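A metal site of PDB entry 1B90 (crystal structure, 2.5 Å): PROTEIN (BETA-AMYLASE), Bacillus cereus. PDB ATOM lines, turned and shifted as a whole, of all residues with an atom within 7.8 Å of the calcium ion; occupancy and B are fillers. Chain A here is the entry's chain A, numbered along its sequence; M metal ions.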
ATOM      1  N   TRP A  52     -22.044   5.583  11.855  1.00  0.00           N
ATOM      2  CA  TRP A  52     -21.232   5.519  13.059  1.00  0.00           C
ATOM      3  C   TRP A  52     -21.220   4.074  13.583  1.00  0.00           C
ATOM      4  O   TRP A  52     -20.196   3.540  14.015  1.00  0.00           O
ATOM      5  CB  TRP A  52     -21.828   6.479  14.080  1.00  0.00           C
ATOM      6  CG  TRP A  52     -20.989   6.781  15.326  1.00  0.00           C
ATOM      7  CD1 TRP A  52     -19.662   6.458  15.420  1.00  0.00           C
ATOM      8  CD2 TRP A  52     -21.469   7.334  16.482  1.00  0.00           C
ATOM      9  NE1 TRP A  52     -19.296   6.804  16.629  1.00  0.00           N
ATOM     10  CE2 TRP A  52     -20.337   7.326  17.299  1.00  0.00           C
ATOM     11  CE3 TRP A  52     -22.689   7.838  16.953  1.00  0.00           C
ATOM     12  CZ2 TRP A  52     -20.400   7.803  18.612  1.00  0.00           C
ATOM     13  CZ3 TRP A  52     -22.752   8.315  18.267  1.00  0.00           C
ATOM     14  CH2 TRP A  52     -21.612   8.302  19.080  1.00  0.00           C
ATOM     15  N   GLU A  56     -17.229   2.851  14.283  1.00  0.00           N
ATOM     16  CA  GLU A  56     -16.641   2.894  15.626  1.00  0.00           C
ATOM     17  C   GLU A  56     -17.501   1.893  16.350  1.00  0.00           C
ATOM     18  O   GLU A  56     -18.065   2.191  17.406  1.00  0.00           O
ATOM     19  CB  GLU A  56     -16.773   4.302  16.241  1.00  0.00           C
ATOM     20  CG  GLU A  56     -15.996   4.610  17.538  1.00  0.00           C
ATOM     21  CD  GLU A  56     -15.985   6.031  18.167  1.00  0.00           C
ATOM     22  OE1 GLU A  56     -16.460   7.030  17.627  1.00  0.00           O
ATOM     23  OE2 GLU A  56     -15.449   6.148  19.262  1.00  0.00           O
ATOM     24  N   GLY A  59     -15.719  -0.634  20.098  1.00  0.00           N
ATOM     25  CA  GLY A  59     -15.526   0.110  21.310  1.00  0.00           C
ATOM     26  C   GLY A  59     -15.136   1.526  21.013  1.00  0.00           C
ATOM     27  O   GLY A  59     -14.998   1.935  19.858  1.00  0.00           O
ATOM     28  N   ASP A  60     -14.947   2.244  22.112  1.00  0.00           N
ATOM     29  CA  ASP A  60     -14.571   3.635  22.042  1.00  0.00           C
ATOM     30  C   ASP A  60     -13.157   3.755  21.498  1.00  0.00           C
ATOM     31  O   ASP A  60     -12.175   3.292  22.072  1.00  0.00           O
ATOM     32  CB  ASP A  60     -14.698   4.232  23.435  1.00  0.00           C
ATOM     33  CG  ASP A  60     -14.651   5.749  23.529  1.00  0.00           C
ATOM     34  OD1 ASP A  60     -14.450   6.456  22.537  1.00  0.00           O
ATOM     35  OD2 ASP A  60     -14.799   6.239  24.635  1.00  0.00           O
ATOM     36  N   GLN A  61     -13.151   4.387  20.324  1.00  0.00           N
ATOM     37  CA  GLN A  61     -11.996   4.687  19.512  1.00  0.00           C
ATOM     38  C   GLN A  61     -11.270   3.518  18.853  1.00  0.00           C
ATOM     39  O   GLN A  61     -10.062   3.550  18.570  1.00  0.00           O
ATOM     40  CB  GLN A  61     -11.029   5.514  20.314  1.00  0.00           C
ATOM     41  CG  GLN A  61     -11.717   6.811  20.624  1.00  0.00           C
ATOM     42  CD  GLN A  61     -10.784   7.984  20.491  1.00  0.00           C
ATOM     43  OE1 GLN A  61     -11.001   8.884  19.677  1.00  0.00           O
ATOM     44  NE2 GLN A  61      -9.713   8.013  21.287  1.00  0.00           N
ATOM     45  N   GLN A  62     -12.060   2.455  18.637  1.00  0.00           N
ATOM     46  CA  GLN A  62     -11.615   1.253  17.938  1.00  0.00           C
ATOM     47  C   GLN A  62     -12.375   1.481  16.612  1.00  0.00           C
ATOM     48  O   GLN A  62     -13.512   1.036  16.408  1.00  0.00           O
ATOM     49  CB  GLN A  62     -12.106  -0.006  18.635  1.00  0.00           C
ATOM     50  CG  GLN A  62     -11.442  -0.398  19.927  1.00  0.00           C
ATOM     51  CD  GLN A  62     -12.046  -1.704  20.441  1.00  0.00           C
ATOM     52  OE1 GLN A  62     -12.854  -1.695  21.375  1.00  0.00           O
ATOM     53  NE2 GLN A  62     -11.701  -2.844  19.826  1.00  0.00           N
ATOM     54  N   PHE A  63     -11.719   2.308  15.804  1.00  0.00           N
ATOM     55  CA  PHE A  63     -12.148   2.780  14.495  1.00  0.00           C
ATOM     56  C   PHE A  63     -11.861   1.972  13.247  1.00  0.00           C
ATOM     57  O   PHE A  63     -10.766   1.445  13.013  1.00  0.00           O
ATOM     58  CB  PHE A  63     -11.567   4.139  14.189  1.00  0.00           C
ATOM     59  CG  PHE A  63     -12.006   5.275  15.052  1.00  0.00           C
ATOM     60  CD1 PHE A  63     -13.311   5.748  14.959  1.00  0.00           C
ATOM     61  CD2 PHE A  63     -11.085   5.866  15.921  1.00  0.00           C
ATOM     62  CE1 PHE A  63     -13.698   6.822  15.770  1.00  0.00           C
ATOM     63  CE2 PHE A  63     -11.496   6.938  16.712  1.00  0.00           C
ATOM     64  CZ  PHE A  63     -12.791   7.416  16.635  1.00  0.00           C
ATOM     65  N   TRP A 106     -21.958   0.611  22.654  1.00  0.00           N
ATOM     66  CA  TRP A 106     -21.199   0.970  23.837  1.00  0.00           C
ATOM     67  C   TRP A 106     -21.443   2.416  24.291  1.00  0.00           C
ATOM     68  O   TRP A 106     -21.022   2.867  25.358  1.00  0.00           O
ATOM     69  CB  TRP A 106     -19.719   0.813  23.582  1.00  0.00           C
ATOM     70  CG  TRP A 106     -19.269   1.609  22.362  1.00  0.00           C
ATOM     71  CD1 TRP A 106     -19.156   0.971  21.164  1.00  0.00           C
ATOM     72  CD2 TRP A 106     -18.949   2.952  22.294  1.00  0.00           C
ATOM     73  NE1 TRP A 106     -18.770   1.891  20.331  1.00  0.00           N
ATOM     74  CE2 TRP A 106     -18.630   3.077  20.935  1.00  0.00           C
ATOM     75  CE3 TRP A 106     -18.881   4.086  23.122  1.00  0.00           C
ATOM     76  CZ2 TRP A 106     -18.247   4.296  20.395  1.00  0.00           C
ATOM     77  CZ3 TRP A 106     -18.492   5.322  22.572  1.00  0.00           C
ATOM     78  CH2 TRP A 106     -18.180   5.415  21.216  1.00  0.00           C
ATOM     79  N   VAL A 107     -22.111   3.205  23.461  1.00  0.00           N
ATOM     80  CA  VAL A 107     -22.330   4.597  23.792  1.00  0.00           C
ATOM     81  C   VAL A 107     -23.287   4.707  24.929  1.00  0.00           C
ATOM     82  O   VAL A 107     -23.005   5.380  25.907  1.00  0.00           O
ATOM     83  CB  VAL A 107     -22.853   5.365  22.553  1.00  0.00           C
ATOM     84  CG1 VAL A 107     -22.872   6.829  22.830  1.00  0.00           C
ATOM     85  CG2 VAL A 107     -21.879   5.275  21.399  1.00  0.00           C
ATOM     86  N   GLN A 110     -22.180   5.228  28.698  1.00  0.00           N
ATOM     87  CA  GLN A 110     -21.376   6.326  29.203  1.00  0.00           C
ATOM     88  C   GLN A 110     -22.085   6.960  30.386  1.00  0.00           C
ATOM     89  O   GLN A 110     -21.384   7.462  31.266  1.00  0.00           O
ATOM     90  CB  GLN A 110     -21.148   7.397  28.142  1.00  0.00           C
ATOM     91  CG  GLN A 110     -20.489   6.877  26.909  1.00  0.00           C
ATOM     92  CD  GLN A 110     -19.282   6.015  27.148  1.00  0.00           C
ATOM     93  OE1 GLN A 110     -19.401   4.823  27.471  1.00  0.00           O
ATOM     94  NE2 GLN A 110     -18.087   6.585  26.992  1.00  0.00           N
ATOM     95  N   VAL A 137     -21.727  14.178  26.283  1.00  0.00           N
ATOM     96  CA  VAL A 137     -21.420  12.949  25.572  1.00  0.00           C
ATOM     97  C   VAL A 137     -21.319  13.296  24.089  1.00  0.00           C
ATOM     98  O   VAL A 137     -20.423  12.791  23.412  1.00  0.00           O
ATOM     99  CB  VAL A 137     -22.498  11.915  25.806  1.00  0.00           C
ATOM    100  CG1 VAL A 137     -22.395  10.725  24.871  1.00  0.00           C
ATOM    101  CG2 VAL A 137     -22.282  11.407  27.205  1.00  0.00           C
ATOM    102  N   LYS A 140     -17.877  14.849  23.368  1.00  0.00           N
ATOM    103  CA  LYS A 140     -16.818  13.883  23.428  1.00  0.00           C
ATOM    104  C   LYS A 140     -16.878  12.981  22.202  1.00  0.00           C
ATOM    105  O   LYS A 140     -16.023  13.105  21.320  1.00  0.00           O
ATOM    106  CB  LYS A 140     -16.940  13.022  24.675  1.00  0.00           C
ATOM    107  CG  LYS A 140     -15.805  11.993  24.742  1.00  0.00           C
ATOM    108  CD  LYS A 140     -16.199  10.779  25.585  1.00  0.00           C
ATOM    109  CE  LYS A 140     -15.173   9.639  25.487  1.00  0.00           C
ATOM    110  NZ  LYS A 140     -15.140   9.017  24.175  1.00  0.00           N
ATOM    111  N   GLU A 141     -17.931  12.155  22.135  1.00  0.00           N
ATOM    112  CA  GLU A 141     -18.117  11.214  21.053  1.00  0.00           C
ATOM    113  C   GLU A 141     -18.153  11.768  19.646  1.00  0.00           C
ATOM    114  O   GLU A 141     -17.501  11.185  18.769  1.00  0.00           O
ATOM    115  CB  GLU A 141     -19.385  10.417  21.315  1.00  0.00           C
ATOM    116  CG  GLU A 141     -19.413   9.567  22.583  1.00  0.00           C
ATOM    117  CD  GLU A 141     -18.183   8.695  22.886  1.00  0.00           C
ATOM    118  OE1 GLU A 141     -17.413   8.317  22.004  1.00  0.00           O
ATOM    119  OE2 GLU A 141     -17.995   8.384  24.056  1.00  0.00           O
ATOM    120  N   TYR A 142     -18.839  12.889  19.367  1.00  0.00           N
ATOM    121  CA  TYR A 142     -18.847  13.380  17.999  1.00  0.00           C
ATOM    122  C   TYR A 142     -17.535  14.013  17.647  1.00  0.00           C
ATOM    123  O   TYR A 142     -17.065  13.723  16.540  1.00  0.00           O
ATOM    124  CB  TYR A 142     -19.905  14.427  17.739  1.00  0.00           C
ATOM    125  CG  TYR A 142     -21.324  13.880  17.566  1.00  0.00           C
ATOM    126  CD1 TYR A 142     -21.777  12.780  18.313  1.00  0.00           C
ATOM    127  CD2 TYR A 142     -22.198  14.559  16.720  1.00  0.00           C
ATOM    128  CE1 TYR A 142     -23.105  12.362  18.238  1.00  0.00           C
ATOM    129  CE2 TYR A 142     -23.535  14.165  16.618  1.00  0.00           C
ATOM    130  CZ  TYR A 142     -23.983  13.070  17.398  1.00  0.00           C
ATOM    131  OH  TYR A 142     -25.322  12.702  17.339  1.00  0.00           O
ATOM    132  N   GLY A 143     -16.898  14.772  18.551  1.00  0.00           N
ATOM    133  CA  GLY A 143     -15.623  15.427  18.255  1.00  0.00           C
ATOM    134  C   GLY A 143     -14.528  14.468  17.796  1.00  0.00           C
ATOM    135  O   GLY A 143     -13.801  14.713  16.825  1.00  0.00           O
ATOM    136  N   GLU A 144     -14.478  13.346  18.530  1.00  0.00           N
ATOM    137  CA  GLU A 144     -13.522  12.281  18.281  1.00  0.00           C
ATOM    138  C   GLU A 144     -13.872  11.671  16.982  1.00  0.00           C
ATOM    139  O   GLU A 144     -12.990  11.628  16.146  1.00  0.00           O
ATOM    140  CB  GLU A 144     -13.586  11.174  19.306  1.00  0.00           C
ATOM    141  CG  GLU A 144     -13.136  11.530  20.741  1.00  0.00           C
ATOM    142  CD  GLU A 144     -13.361  10.395  21.733  1.00  0.00           C
ATOM    143  OE1 GLU A 144     -14.113   9.451  21.430  1.00  0.00           O
ATOM    144  OE2 GLU A 144     -12.776  10.439  22.817  1.00  0.00           O
ATOM    145  N   LEU A 145     -15.128  11.237  16.778  1.00  0.00           N
ATOM    146  CA  LEU A 145     -15.543  10.659  15.512  1.00  0.00           C
ATOM    147  C   LEU A 145     -15.171  11.520  14.311  1.00  0.00           C
ATOM    148  O   LEU A 145     -14.479  11.067  13.392  1.00  0.00           O
ATOM    149  CB  LEU A 145     -17.054  10.470  15.437  1.00  0.00           C
ATOM    150  CG  LEU A 145     -17.550   9.752  14.168  1.00  0.00           C
ATOM    151  CD1 LEU A 145     -17.001   8.351  14.179  1.00  0.00           C
ATOM    152  CD2 LEU A 145     -19.038   9.640  14.116  1.00  0.00           C
HETATM  153 CA    CA M   1     -15.471   8.073  20.670  1.00  0.00          CA
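OE2 of Glu 144 is in salt-bridge range of NZ of Lys 140 (3.1 Å). The side-chain carboxylate of Glu 141 lies within salt-bridge range of the side-chain amino group of Lys 140 (2.9 Å). NE2 of Gln 110 sits at hydrogen-bond distance from OE2 of Glu 141 (3.4 Å). The indole nitrogen of Trp 106 is in hydrogen-bond range of the backbone carbonyl oxygen of Glu 56 (3.0 Å). OE2 of Glu 56 sits close to N of Gln 61 (3.1 Å). The indole nitrogen (NE1) of Trp 52 lies within hydrogen-bond range of the side-chain carboxylate (OE1) of Glu 56 (3.0 Å). The side-chain amino group (NZ) of Lys 140 is in salt-bridge range of the side-chain carboxylate (OD2) of Asp 60, 2.8 Å away. The backbone carbonyl oxygen (O) of Trp 106 sits close to the side-chain amide oxygen (OE1) of Gln 110.
Gln 61 touches the calcium ion (CG to CA, 3.96 Å). Trp 106 touches the calcium ion. Lys 140 touches the calcium ion (NZ to CA, 3.6 Å). Within 4 Å of the calcium ion: Glu 56, Asp 60, Gln 61, Trp 106, Lys 140, Glu 141 and Glu 144. The nearest printed residue that does not touch the calcium ion is Phe 63 (4.9 Å).
The calcium ion is bound by the side-chain carboxylate (OE1) of Glu 144, the side-chain carboxylate (OE1) of Glu 141, the side-chain carboxylate (OE2) of Glu 56 and the side-chain carboxylate (OD1) of Asp 60.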
